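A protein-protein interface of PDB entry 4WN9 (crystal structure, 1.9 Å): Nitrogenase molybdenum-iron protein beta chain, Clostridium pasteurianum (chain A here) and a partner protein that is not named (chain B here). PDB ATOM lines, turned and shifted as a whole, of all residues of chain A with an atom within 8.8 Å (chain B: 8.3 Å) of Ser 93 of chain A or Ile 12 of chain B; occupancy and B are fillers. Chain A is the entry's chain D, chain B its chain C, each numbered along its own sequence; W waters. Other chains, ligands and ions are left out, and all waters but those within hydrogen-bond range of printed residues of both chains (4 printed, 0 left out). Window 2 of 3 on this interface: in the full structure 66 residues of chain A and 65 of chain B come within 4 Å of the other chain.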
ATOM      1  N   LYS A  85      17.739  14.902  14.376  1.00  0.00           N
ATOM      2  CA  LYS A  85      16.643  13.971  14.638  1.00  0.00           C
ATOM      3  C   LYS A  85      17.157  12.534  14.581  1.00  0.00           C
ATOM      4  O   LYS A  85      16.789  11.703  15.390  1.00  0.00           O
ATOM      5  CB  LYS A  85      15.500  14.175  13.635  1.00  0.00           C
ATOM      6  CG  LYS A  85      14.686  15.433  13.863  1.00  0.00           C
ATOM      7  CD  LYS A  85      13.653  15.620  12.760  1.00  0.00           C
ATOM      8  CE  LYS A  85      13.175  17.063  12.671  1.00  0.00           C
ATOM      9  NZ  LYS A  85      12.384  17.314  11.435  1.00  0.00           N
ATOM     10  N   THR A  86      18.014  12.258  13.606  1.00  0.00           N
ATOM     11  CA  THR A  86      18.681  10.976  13.510  1.00  0.00           C
ATOM     12  C   THR A  86      19.476  10.729  14.799  1.00  0.00           C
ATOM     13  O   THR A  86      19.441   9.634  15.368  1.00  0.00           O
ATOM     14  CB  THR A  86      19.637  10.964  12.308  1.00  0.00           C
ATOM     15  OG1 THR A  86      18.901  11.227  11.100  1.00  0.00           O
ATOM     16  CG2 THR A  86      20.364   9.627  12.188  1.00  0.00           C
ATOM     17  N   ALA A  87      20.170  11.761  15.270  1.00  0.00           N
ATOM     18  CA  ALA A  87      20.998  11.640  16.477  1.00  0.00           C
ATOM     19  C   ALA A  87      20.202  11.263  17.721  1.00  0.00           C
ATOM     20  O   ALA A  87      20.589  10.352  18.458  1.00  0.00           O
ATOM     21  CB  ALA A  87      21.768  12.924  16.719  1.00  0.00           C
ATOM     22  N   VAL A  88      19.090  11.951  17.962  1.00  0.00           N
ATOM     23  CA  VAL A  88      18.301  11.679  19.157  1.00  0.00           C
ATOM     24  C   VAL A  88      17.825  10.233  19.206  1.00  0.00           C
ATOM     25  O   VAL A  88      17.820   9.623  20.272  1.00  0.00           O
ATOM     26  CB  VAL A  88      17.097  12.632  19.283  1.00  0.00           C
ATOM     27  CG1 VAL A  88      16.135  12.148  20.364  1.00  0.00           C
ATOM     28  CG2 VAL A  88      17.567  14.045  19.588  1.00  0.00           C
ATOM     29  N   LYS A  89      17.424   9.669  18.067  1.00  0.00           N
ATOM     30  CA  LYS A  89      16.963   8.271  18.059  1.00  0.00           C
ATOM     31  C   LYS A  89      18.120   7.313  18.350  1.00  0.00           C
ATOM     32  O   LYS A  89      17.953   6.292  19.005  1.00  0.00           O
ATOM     33  CB  LYS A  89      16.331   7.896  16.712  1.00  0.00           C
ATOM     34  CG  LYS A  89      15.129   8.743  16.314  1.00  0.00           C
ATOM     35  CD  LYS A  89      14.634   8.399  14.918  1.00  0.00           C
ATOM     36  CE  LYS A  89      13.763   9.518  14.373  1.00  0.00           C
ATOM     37  NZ  LYS A  89      13.140   9.164  13.067  1.00  0.00           N
ATOM     38  N   ASN A  90      19.297   7.635  17.836  1.00  0.00           N
ATOM     39  CA  ASN A  90      20.457   6.810  18.097  1.00  0.00           C
ATOM     40  C   ASN A  90      20.947   6.955  19.530  1.00  0.00           C
ATOM     41  O   ASN A  90      21.335   5.976  20.155  1.00  0.00           O
ATOM     42  CB  ASN A  90      21.555   7.108  17.088  1.00  0.00           C
ATOM     43  CG  ASN A  90      21.333   6.379  15.782  1.00  0.00           C
ATOM     44  OD1 ASN A  90      21.299   5.143  15.742  1.00  0.00           O
ATOM     45  ND2 ASN A  90      21.180   7.132  14.708  1.00  0.00           N
ATOM     46  N   ILE A  91      20.914   8.174  20.050  1.00  0.00           N
ATOM     47  CA  ILE A  91      21.294   8.430  21.437  1.00  0.00           C
ATOM     48  C   ILE A  91      20.417   7.699  22.449  1.00  0.00           C
ATOM     49  O   ILE A  91      20.934   6.997  23.321  1.00  0.00           O
ATOM     50  CB  ILE A  91      21.236   9.928  21.741  1.00  0.00           C
ATOM     51  CG1 ILE A  91      22.333  10.646  20.946  1.00  0.00           C
ATOM     52  CG2 ILE A  91      21.387  10.162  23.239  1.00  0.00           C
ATOM     53  CD1 ILE A  91      22.127  12.136  20.819  1.00  0.00           C
ATOM     54  N   PHE A  92      19.099   7.877  22.368  1.00  0.00           N
ATOM     55  CA  PHE A  92      18.218   7.276  23.369  1.00  0.00           C
ATOM     56  C   PHE A  92      18.253   5.752  23.323  1.00  0.00           C
ATOM     57  O   PHE A  92      18.250   5.104  24.362  1.00  0.00           O
ATOM     58  CB  PHE A  92      16.778   7.768  23.230  1.00  0.00           C
ATOM     59  CG  PHE A  92      16.535   9.080  23.886  1.00  0.00           C
ATOM     60  CD1 PHE A  92      16.713   9.223  25.254  1.00  0.00           C
ATOM     61  CD2 PHE A  92      16.150  10.178  23.140  1.00  0.00           C
ATOM     62  CE1 PHE A  92      16.506  10.431  25.862  1.00  0.00           C
ATOM     63  CE2 PHE A  92      15.942  11.400  23.738  1.00  0.00           C
ATOM     64  CZ  PHE A  92      16.119  11.527  25.105  1.00  0.00           C
ATOM     65  N   SER A  93      18.312   5.184  22.122  1.00  0.00           N
ATOM     66  CA  SER A  93      18.313   3.729  21.968  1.00  0.00           C
ATOM     67  C   SER A  93      19.650   3.091  22.333  1.00  0.00           C
ATOM     68  O   SER A  93      19.681   2.044  22.975  1.00  0.00           O
ATOM     69  CB  SER A  93      17.970   3.339  20.530  1.00  0.00           C
ATOM     70  OG  SER A  93      18.994   3.756  19.639  1.00  0.00           O
ATOM     71  N   LEU A  94      20.751   3.709  21.914  1.00  0.00           N
ATOM     72  CA  LEU A  94      22.072   3.145  22.195  1.00  0.00           C
ATOM     73  C   LEU A  94      22.614   3.533  23.553  1.00  0.00           C
ATOM     74  O   LEU A  94      23.387   2.798  24.133  1.00  0.00           O
ATOM     75  CB  LEU A  94      23.100   3.604  21.170  1.00  0.00           C
ATOM     76  CG  LEU A  94      23.220   2.806  19.876  1.00  0.00           C
ATOM     77  CD1 LEU A  94      24.079   3.605  18.915  1.00  0.00           C
ATOM     78  CD2 LEU A  94      23.801   1.420  20.125  1.00  0.00           C
ATOM     79  N   TYR A  95      22.244   4.702  24.050  1.00  0.00           N
ATOM     80  CA  TYR A  95      22.991   5.258  25.167  1.00  0.00           C
ATOM     81  C   TYR A  95      22.132   5.670  26.344  1.00  0.00           C
ATOM     82  O   TYR A  95      22.625   5.768  27.470  1.00  0.00           O
ATOM     83  CB  TYR A  95      23.853   6.410  24.665  1.00  0.00           C
ATOM     84  CG  TYR A  95      24.887   5.947  23.664  1.00  0.00           C
ATOM     85  CD1 TYR A  95      25.760   4.918  23.971  1.00  0.00           C
ATOM     86  CD2 TYR A  95      24.977   6.517  22.404  1.00  0.00           C
ATOM     87  CE1 TYR A  95      26.701   4.479  23.065  1.00  0.00           C
ATOM     88  CE2 TYR A  95      25.911   6.081  21.494  1.00  0.00           C
ATOM     89  CZ  TYR A  95      26.771   5.055  21.823  1.00  0.00           C
ATOM     90  OH  TYR A  95      27.736   4.610  20.923  1.00  0.00           O
ATOM     91  N   ASN A  96      20.851   5.919  26.076  1.00  0.00           N
ATOM     92  CA  ASN A  96      19.829   5.998  27.120  1.00  0.00           C
ATOM     93  C   ASN A  96      20.120   6.994  28.237  1.00  0.00           C
ATOM     94  O   ASN A  96      19.968   6.660  29.403  1.00  0.00           O
ATOM     95  CB  ASN A  96      19.601   4.608  27.725  1.00  0.00           C
ATOM     96  CG  ASN A  96      18.432   4.565  28.698  1.00  0.00           C
ATOM     97  OD1 ASN A  96      17.400   5.222  28.507  1.00  0.00           O
ATOM     98  ND2 ASN A  96      18.584   3.776  29.748  1.00  0.00           N
ATOM     99  N   PRO A  97      20.515   8.229  27.885  1.00  0.00           N
ATOM    100  CA  PRO A  97      20.451   9.279  28.904  1.00  0.00           C
ATOM    101  C   PRO A  97      19.008   9.536  29.342  1.00  0.00           C
ATOM    102  O   PRO A  97      18.069   9.165  28.620  1.00  0.00           O
ATOM    103  CB  PRO A  97      20.965  10.499  28.159  1.00  0.00           C
ATOM    104  CG  PRO A  97      20.541  10.248  26.747  1.00  0.00           C
ATOM    105  CD  PRO A  97      20.759   8.790  26.548  1.00  0.00           C
ATOM    106  N   ILE A 100      19.095  14.820  27.125  1.00  0.00           N
ATOM    107  CA  ILE A 100      20.051  15.259  26.133  1.00  0.00           C
ATOM    108  C   ILE A 100      20.083  16.782  26.171  1.00  0.00           C
ATOM    109  O   ILE A 100      19.058  17.453  25.983  1.00  0.00           O
ATOM    110  CB  ILE A 100      19.665  14.764  24.742  1.00  0.00           C
ATOM    111  CG1 ILE A 100      19.592  13.235  24.730  1.00  0.00           C
ATOM    112  CG2 ILE A 100      20.655  15.252  23.698  1.00  0.00           C
ATOM    113  CD1 ILE A 100      19.131  12.662  23.402  1.00  0.00           C
ATOM    114  N   SER A 127       9.767  10.973  18.769  1.00  0.00           N
ATOM    115  CA  SER A 127      11.185  10.612  18.734  1.00  0.00           C
ATOM    116  C   SER A 127      11.816  10.668  20.134  1.00  0.00           C
ATOM    117  O   SER A 127      12.941  10.227  20.320  1.00  0.00           O
ATOM    118  CB  SER A 127      11.954  11.540  17.789  1.00  0.00           C
ATOM    119  OG  SER A 127      11.256  11.755  16.573  1.00  0.00           O
ATOM    120  N   PRO A 129      11.374   9.328  23.818  1.00  0.00           N
ATOM    121  CA  PRO A 129      10.702   8.373  24.693  1.00  0.00           C
ATOM    122  C   PRO A 129      10.042   9.017  25.911  1.00  0.00           C
ATOM    123  O   PRO A 129      10.491  10.052  26.396  1.00  0.00           O
ATOM    124  CB  PRO A 129      11.838   7.449  25.140  1.00  0.00           C
ATOM    125  CG  PRO A 129      12.841   7.502  24.033  1.00  0.00           C
ATOM    126  CD  PRO A 129      12.715   8.865  23.406  1.00  0.00           C
ATOM    127  N   LYS A 132      11.683  11.133  29.157  1.00  0.00           N
ATOM    128  CA  LYS A 132      13.021  11.531  28.720  1.00  0.00           C
ATOM    129  C   LYS A 132      12.937  12.962  28.255  1.00  0.00           C
ATOM    130  O   LYS A 132      11.882  13.402  27.816  1.00  0.00           O
ATOM    131  CB  LYS A 132      13.503  10.684  27.540  1.00  0.00           C
ATOM    132  CG  LYS A 132      13.604   9.192  27.787  1.00  0.00           C
ATOM    133  CD  LYS A 132      14.736   8.879  28.744  1.00  0.00           C
ATOM    134  CE  LYS A 132      14.946   7.382  28.847  1.00  0.00           C
ATOM    135  NZ  LYS A 132      16.201   7.079  29.573  1.00  0.00           N
ATOM    136  N   TYR A 219      27.154   7.168  32.765  1.00  0.00           N
ATOM    137  CA  TYR A 219      26.643   8.325  33.489  1.00  0.00           C
ATOM    138  C   TYR A 219      27.037   8.170  34.949  1.00  0.00           C
ATOM    139  O   TYR A 219      26.402   7.415  35.689  1.00  0.00           O
ATOM    140  CB  TYR A 219      25.118   8.512  33.304  1.00  0.00           C
ATOM    141  CG  TYR A 219      24.714   8.506  31.844  1.00  0.00           C
ATOM    142  CD1 TYR A 219      25.109   9.523  30.992  1.00  0.00           C
ATOM    143  CD2 TYR A 219      23.981   7.463  31.310  1.00  0.00           C
ATOM    144  CE1 TYR A 219      24.784   9.502  29.652  1.00  0.00           C
ATOM    145  CE2 TYR A 219      23.645   7.434  29.971  1.00  0.00           C
ATOM    146  CZ  TYR A 219      24.045   8.461  29.146  1.00  0.00           C
ATOM    147  OH  TYR A 219      23.720   8.439  27.799  1.00  0.00           O
ATOM    148  N   LEU B   8      26.184  -5.660  16.608  1.00  0.00           N
ATOM    149  CA  LEU B   8      25.100  -5.066  15.830  1.00  0.00           C
ATOM    150  C   LEU B   8      23.773  -5.081  16.580  1.00  0.00           C
ATOM    151  O   LEU B   8      22.882  -4.291  16.290  1.00  0.00           O
ATOM    152  CB  LEU B   8      24.943  -5.798  14.497  1.00  0.00           C
ATOM    153  CG  LEU B   8      26.043  -5.610  13.448  1.00  0.00           C
ATOM    154  CD1 LEU B   8      25.720  -6.428  12.207  1.00  0.00           C
ATOM    155  CD2 LEU B   8      26.232  -4.136  13.102  1.00  0.00           C
ATOM    156  N   GLU B   9      23.656  -5.964  17.559  1.00  0.00           N
ATOM    157  CA  GLU B   9      22.384  -6.179  18.266  1.00  0.00           C
ATOM    158  C   GLU B   9      21.572  -4.934  18.628  1.00  0.00           C
ATOM    159  O   GLU B   9      20.412  -4.819  18.250  1.00  0.00           O
ATOM    160  CB  GLU B   9      22.621  -7.011  19.535  1.00  0.00           C
ATOM    161  CG  GLU B   9      21.928  -8.361  19.511  1.00  0.00           C
ATOM    162  CD  GLU B   9      20.417  -8.220  19.526  1.00  0.00           C
ATOM    163  OE1 GLU B   9      19.755  -8.576  18.520  1.00  0.00           O
ATOM    164  OE2 GLU B   9      19.891  -7.722  20.544  1.00  0.00           O
ATOM    165  N   LYS B  10      22.167  -4.010  19.369  1.00  0.00           N
ATOM    166  CA  LYS B  10      21.417  -2.905  19.958  1.00  0.00           C
ATOM    167  C   LYS B  10      21.093  -1.768  18.972  1.00  0.00           C
ATOM    168  O   LYS B  10      20.343  -0.841  19.293  1.00  0.00           O
ATOM    169  CB  LYS B  10      22.226  -2.349  21.139  1.00  0.00           C
ATOM    170  CG  LYS B  10      21.426  -1.598  22.187  1.00  0.00           C
ATOM    171  CD  LYS B  10      22.217  -1.473  23.483  1.00  0.00           C
ATOM    172  CE  LYS B  10      21.573  -0.471  24.431  1.00  0.00           C
ATOM    173  NZ  LYS B  10      22.592   0.352  25.154  1.00  0.00           N
ATOM    174  N   TYR B  11      21.677  -1.811  17.785  1.00  0.00           N
ATOM    175  CA  TYR B  11      21.464  -0.739  16.821  1.00  0.00           C
ATOM    176  C   TYR B  11      20.009  -0.744  16.370  1.00  0.00           C
ATOM    177  O   TYR B  11      19.431  -1.807  16.176  1.00  0.00           O
ATOM    178  CB  TYR B  11      22.337  -0.953  15.584  1.00  0.00           C
ATOM    179  CG  TYR B  11      23.795  -0.589  15.714  1.00  0.00           C
ATOM    180  CD1 TYR B  11      24.193   0.609  16.291  1.00  0.00           C
ATOM    181  CD2 TYR B  11      24.776  -1.429  15.205  1.00  0.00           C
ATOM    182  CE1 TYR B  11      25.532   0.953  16.372  1.00  0.00           C
ATOM    183  CE2 TYR B  11      26.117  -1.098  15.282  1.00  0.00           C
ATOM    184  CZ  TYR B  11      26.497   0.100  15.873  1.00  0.00           C
ATOM    185  OH  TYR B  11      27.844   0.434  15.943  1.00  0.00           O
ATOM    186  N   ILE B  12      19.410   0.425  16.189  1.00  0.00           N
ATOM    187  CA  ILE B  12      18.080   0.467  15.605  1.00  0.00           C
ATOM    188  C   ILE B  12      18.205  -0.016  14.152  1.00  0.00           C
ATOM    189  O   ILE B  12      19.297   0.047  13.565  1.00  0.00           O
ATOM    190  CB  ILE B  12      17.445   1.867  15.694  1.00  0.00           C
ATOM    191  CG1 ILE B  12      18.255   2.878  14.882  1.00  0.00           C
ATOM    192  CG2 ILE B  12      17.337   2.308  17.154  1.00  0.00           C
ATOM    193  CD1 ILE B  12      17.766   4.308  14.976  1.00  0.00           C
ATOM    194  N   PRO B  13      17.094  -0.510  13.566  1.00  0.00           N
ATOM    195  CA  PRO B  13      17.145  -1.108  12.226  1.00  0.00           C
ATOM    196  C   PRO B  13      17.873  -0.292  11.155  1.00  0.00           C
ATOM    197  O   PRO B  13      18.763  -0.816  10.502  1.00  0.00           O
ATOM    198  CB  PRO B  13      15.662  -1.311  11.885  1.00  0.00           C
ATOM    199  CG  PRO B  13      15.039  -1.613  13.216  1.00  0.00           C
ATOM    200  CD  PRO B  13      15.776  -0.729  14.203  1.00  0.00           C
ATOM    201  N   LYS B  14      17.527   0.975  10.975  1.00  0.00           N
ATOM    202  CA  LYS B  14      18.230   1.777   9.977  1.00  0.00           C
ATOM    203  C   LYS B  14      19.743   1.709  10.263  1.00  0.00           C
ATOM    204  O   LYS B  14      20.557   1.380   9.392  1.00  0.00           O
ATOM    205  CB  LYS B  14      17.740   3.226  10.002  1.00  0.00           C
ATOM    206  CG  LYS B  14      18.048   4.033   8.744  1.00  0.00           C
ATOM    207  CD  LYS B  14      18.718   5.375   9.052  1.00  0.00           C
ATOM    208  CE  LYS B  14      20.195   5.181   9.436  1.00  0.00           C
ATOM    209  NZ  LYS B  14      20.962   6.413   9.826  1.00  0.00           N
ATOM    210  N   THR B  15      20.101   2.006  11.508  1.00  0.00           N
ATOM    211  CA  THR B  15      21.505   2.070  11.942  1.00  0.00           C
ATOM    212  C   THR B  15      22.187   0.724  11.760  1.00  0.00           C
ATOM    213  O   THR B  15      23.288   0.627  11.215  1.00  0.00           O
ATOM    214  CB  THR B  15      21.554   2.531  13.416  1.00  0.00           C
ATOM    215  OG1 THR B  15      20.901   3.800  13.504  1.00  0.00           O
ATOM    216  CG2 THR B  15      22.978   2.679  13.930  1.00  0.00           C
ATOM    217  N   LYS B  16      21.500  -0.325  12.180  1.00  0.00           N
ATOM    218  CA  LYS B  16      22.037  -1.666  12.072  1.00  0.00           C
ATOM    219  C   LYS B  16      22.438  -1.969  10.638  1.00  0.00           C
ATOM    220  O   LYS B  16      23.496  -2.543  10.384  1.00  0.00           O
ATOM    221  CB  LYS B  16      21.005  -2.679  12.556  1.00  0.00           C
ATOM    222  CG  LYS B  16      21.546  -4.092  12.573  1.00  0.00           C
ATOM    223  CD  LYS B  16      20.712  -4.990  13.448  1.00  0.00           C
ATOM    224  CE  LYS B  16      21.113  -6.442  13.250  1.00  0.00           C
ATOM    225  NZ  LYS B  16      20.268  -7.363  14.063  1.00  0.00           N
ATOM    226  N   LYS B  17      21.583  -1.557   9.706  1.00  0.00           N
ATOM    227  CA  LYS B  17      21.775  -1.807   8.282  1.00  0.00           C
ATOM    228  C   LYS B  17      22.984  -1.049   7.735  1.00  0.00           C
ATOM    229  O   LYS B  17      23.820  -1.636   7.051  1.00  0.00           O
ATOM    230  CB  LYS B  17      20.501  -1.414   7.517  1.00  0.00           C
ATOM    231  CG  LYS B  17      20.527  -1.764   6.035  1.00  0.00           C
ATOM    232  CD  LYS B  17      19.122  -1.874   5.448  1.00  0.00           C
ATOM    233  CE  LYS B  17      18.507  -0.513   5.164  1.00  0.00           C
ATOM    234  NZ  LYS B  17      17.964   0.155   6.382  1.00  0.00           N
ATOM    235  N   THR B  18      23.085   0.240   8.056  1.00  0.00           N
ATOM    236  CA  THR B  18      24.236   1.063   7.639  1.00  0.00           C
ATOM    237  C   THR B  18      25.563   0.553   8.219  1.00  0.00           C
ATOM    238  O   THR B  18      26.547   0.450   7.492  1.00  0.00           O
ATOM    239  CB  THR B  18      24.084   2.544   8.054  1.00  0.00           C
ATOM    240  OG1 THR B  18      24.003   2.640   9.482  1.00  0.00           O
ATOM    241  CG2 THR B  18      22.840   3.168   7.439  1.00  0.00           C
ATOM    242  N   ARG B  19      25.573   0.233   9.517  1.00  0.00           N
ATOM    243  CA  ARG B  19      26.806  -0.169  10.232  1.00  0.00           C
ATOM    244  C   ARG B  19      27.302  -1.571   9.872  1.00  0.00           C
ATOM    245  O   ARG B  19      28.512  -1.839   9.894  1.00  0.00           O
ATOM    246  CB  ARG B  19      26.603  -0.092  11.754  1.00  0.00           C
ATOM    247  CG  ARG B  19      26.438   1.319  12.311  1.00  0.00           C
ATOM    248  CD  ARG B  19      27.726   2.114  12.242  1.00  0.00           C
ATOM    249  NE  ARG B  19      28.761   1.484  13.042  1.00  0.00           N
ATOM    250  CZ  ARG B  19      30.061   1.481  12.751  1.00  0.00           C
ATOM    251  NH1 ARG B  19      30.531   2.079  11.665  1.00  0.00           N
ATOM    252  NH2 ARG B  19      30.901   0.879  13.569  1.00  0.00           N
ATOM    253  N   VAL B  42      27.407   8.241  11.388  1.00  0.00           N
ATOM    254  CA  VAL B  42      26.040   8.257  11.874  1.00  0.00           C
ATOM    255  C   VAL B  42      25.900   9.270  13.027  1.00  0.00           C
ATOM    256  O   VAL B  42      26.629   9.179  14.026  1.00  0.00           O
ATOM    257  CB  VAL B  42      25.582   6.874  12.348  1.00  0.00           C
ATOM    258  CG1 VAL B  42      24.178   6.939  12.952  1.00  0.00           C
ATOM    259  CG2 VAL B  42      25.635   5.870  11.198  1.00  0.00           C
ATOM    260  N   PRO B  43      24.958  10.234  12.899  1.00  0.00           N
ATOM    261  CA  PRO B  43      24.691  11.216  13.958  1.00  0.00           C
ATOM    262  C   PRO B  43      24.291  10.554  15.259  1.00  0.00           C
ATOM    263  O   PRO B  43      23.443   9.654  15.239  1.00  0.00           O
ATOM    264  CB  PRO B  43      23.500  12.016  13.410  1.00  0.00           C
ATOM    265  CG  PRO B  43      23.550  11.839  11.934  1.00  0.00           C
ATOM    266  CD  PRO B  43      24.096  10.457  11.720  1.00  0.00           C
ATOM    267  N   GLY B  44      24.906  10.977  16.371  1.00  0.00           N
ATOM    268  CA  GLY B  44      24.544  10.505  17.714  1.00  0.00           C
ATOM    269  C   GLY B  44      25.153   9.175  18.149  1.00  0.00           C
ATOM    270  O   GLY B  44      24.825   8.631  19.201  1.00  0.00           O
ATOM    271  N   ILE B  45      26.038   8.639  17.339  1.00  0.00           N
ATOM    272  CA  ILE B  45      26.598   7.311  17.589  1.00  0.00           C
ATOM    273  C   ILE B  45      27.823   7.329  18.549  1.00  0.00           C
ATOM    274  O   ILE B  45      28.237   6.280  19.059  1.00  0.00           O
ATOM    275  CB  ILE B  45      26.963   6.684  16.228  1.00  0.00           C
ATOM    276  CG1 ILE B  45      26.803   5.171  16.264  1.00  0.00           C
ATOM    277  CG2 ILE B  45      28.338   7.135  15.772  1.00  0.00           C
ATOM    278  CD1 ILE B  45      25.360   4.723  16.194  1.00  0.00           C
ATOM    279  N   HIS B 445      29.546   2.371  21.719  1.00  0.00           N
ATOM    280  CA  HIS B 445      28.791   1.107  21.769  1.00  0.00           C
ATOM    281  C   HIS B 445      29.629  -0.084  21.299  1.00  0.00           C
ATOM    282  O   HIS B 445      29.791  -1.064  22.035  1.00  0.00           O
ATOM    283  CB  HIS B 445      27.506   1.160  20.927  1.00  0.00           C
ATOM    284  CG  HIS B 445      26.887  -0.189  20.729  1.00  0.00           C
ATOM    285  ND1 HIS B 445      26.120  -0.801  21.696  1.00  0.00           N
ATOM    286  CD2 HIS B 445      26.968  -1.064  19.699  1.00  0.00           C
ATOM    287  CE1 HIS B 445      25.737  -1.987  21.262  1.00  0.00           C
ATOM    288  NE2 HIS B 445      26.239  -2.171  20.054  1.00  0.00           N
HETATM  289  O   HOH W   1      20.252   6.140  12.332  1.00  0.00           O
HETATM  290  O   HOH W   2      25.474   0.631  23.851  1.00  0.00           O
HETATM  291  O   HOH W   3      22.189   2.132  27.180  1.00  0.00           O
HETATM  292  O   HOH W   4      21.003   2.964  17.139  1.00  0.00           O
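O of Leu 94 of chain A sits at hydrogen-bond distance from NZ of Lys 10 of chain B (2.8 Å). The backbone carbonyl oxygen of Pro 43 of chain B lies within hydrogen-bond range of the side-chain amide nitrogen of Asn 90 of chain A (3.4 Å). The backbone carbonyl oxygen (O) of Ile 45 of chain B sits at hydrogen-bond distance from the side-chain hydroxyl (OH) of Tyr 95 of chain A, 2.6 Å away. The side-chain hydroxyl of Tyr 95 of chain A lies within hydrogen-bond range of the backbone NH of His 445 of chain B (3.0 Å). OG1 of Thr 15 of chain B is in hydrogen-bond range of OD1 of Asn 90 of chain A (2.6 Å).
The side-chain hydroxyl (OH) of Tyr 11 of chain B sits at hydrogen-bond distance from the guanidinium group (NE) of Arg 19 of chain B, at 3.2 Å. O of Tyr 95 of chain A lies within hydrogen-bond range of OH of Tyr 219 of chain A (2.9 Å). O of Asn 90 of chain A is in hydrogen-bond range of OG of Ser 93 of chain A (3.3 Å). The backbone carbonyl oxygen of Thr 86 of chain A is in hydrogen-bond range of the side-chain amide nitrogen of Asn 90 of chain A, at 3.1 Å. O of Ile 91 of chain A sits at hydrogen-bond distance from N of Asn 96 of chain A (3.0 Å). O of Thr 15 of chain B lies within hydrogen-bond range of OG1 of Thr 18 of chain B, at 2.8 Å.
Among the printed residues, merely in contact across the chains: Leu 94 of chain A with Ile 45 of chain B, Ser 93 of chain A with Ile 12 of chain B, Ala 87 of chain A with Pro 43 of chain B, Ser 93 of chain A with Lys 10 of chain B, Asn 90 of chain A with Val 42 of chain B, Leu 94 of chain A with His 445 of chain B, Tyr 95 of chain A with Gly 44 of chain B, Ile 91 of chain A with Gly 44 of chain B, Ala 87 of chain A with Gly 44 of chain B, Asn 90 of chain A with Ile 12 of chain B, Thr 86 of chain A with Pro 43 of chain B and Leu 94 of chain A with Tyr 11 of chain B.
Ser 93 of chain A touches just these residues of chain B: Lys 10 and Ile 12. Of the printed residues of chain A, Tyr 11 of chain B touches Leu 94. Of chain A, only Asn 90 and Ser 93 come within 4 Å of Ile 12 of chain B. Printed residues of chain A within 4 Å of Pro 43 of chain B: Thr 86 (3.9 Å), Ala 87 (3.4 Å) and Asn 90 (3.4 Å).
Hydrophobic or aromatic side chains of chain A that line the printed part of chain B: Ala 87, Ile 91, Leu 94 and Tyr 95. Of the 17 printed residues of chain B, 9 touch a printed residue of chain A. Printed residues of chain B that touch a printed residue of chain A: Lys 10, Tyr 11, Ile 12, Thr 15, Val 42, Pro 43, Gly 44, Ile 45 and His 445. Among the printed residues, 17 pairs touch across the chains.
Water W4 lies within hydrogen-bond range of OD1 of Asn 90 of chain A (2.6 Å), N of Ile 12 of chain B (3.1 Å) and OG of Ser 93 of chain A (3.3 Å). Water W1 lies within hydrogen-bond range of NZ of Lys 14 of chain B (2.6 Å), OG1 of Thr 15 of chain B (2.7 Å) and ND2 of Asn 90 of chain A (2.7 Å). Water W2 lies within hydrogen-bond range of ND1 of His 445 of chain B (2.7 Å), O of Leu 94 of chain A (3.0 Å) and NZ of Lys 10 of chain B (3.2 Å). Water W3 bridges the side-chain amino group of Lys 10 of chain B and the backbone carbonyl oxygen of Leu 94 of chain A.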
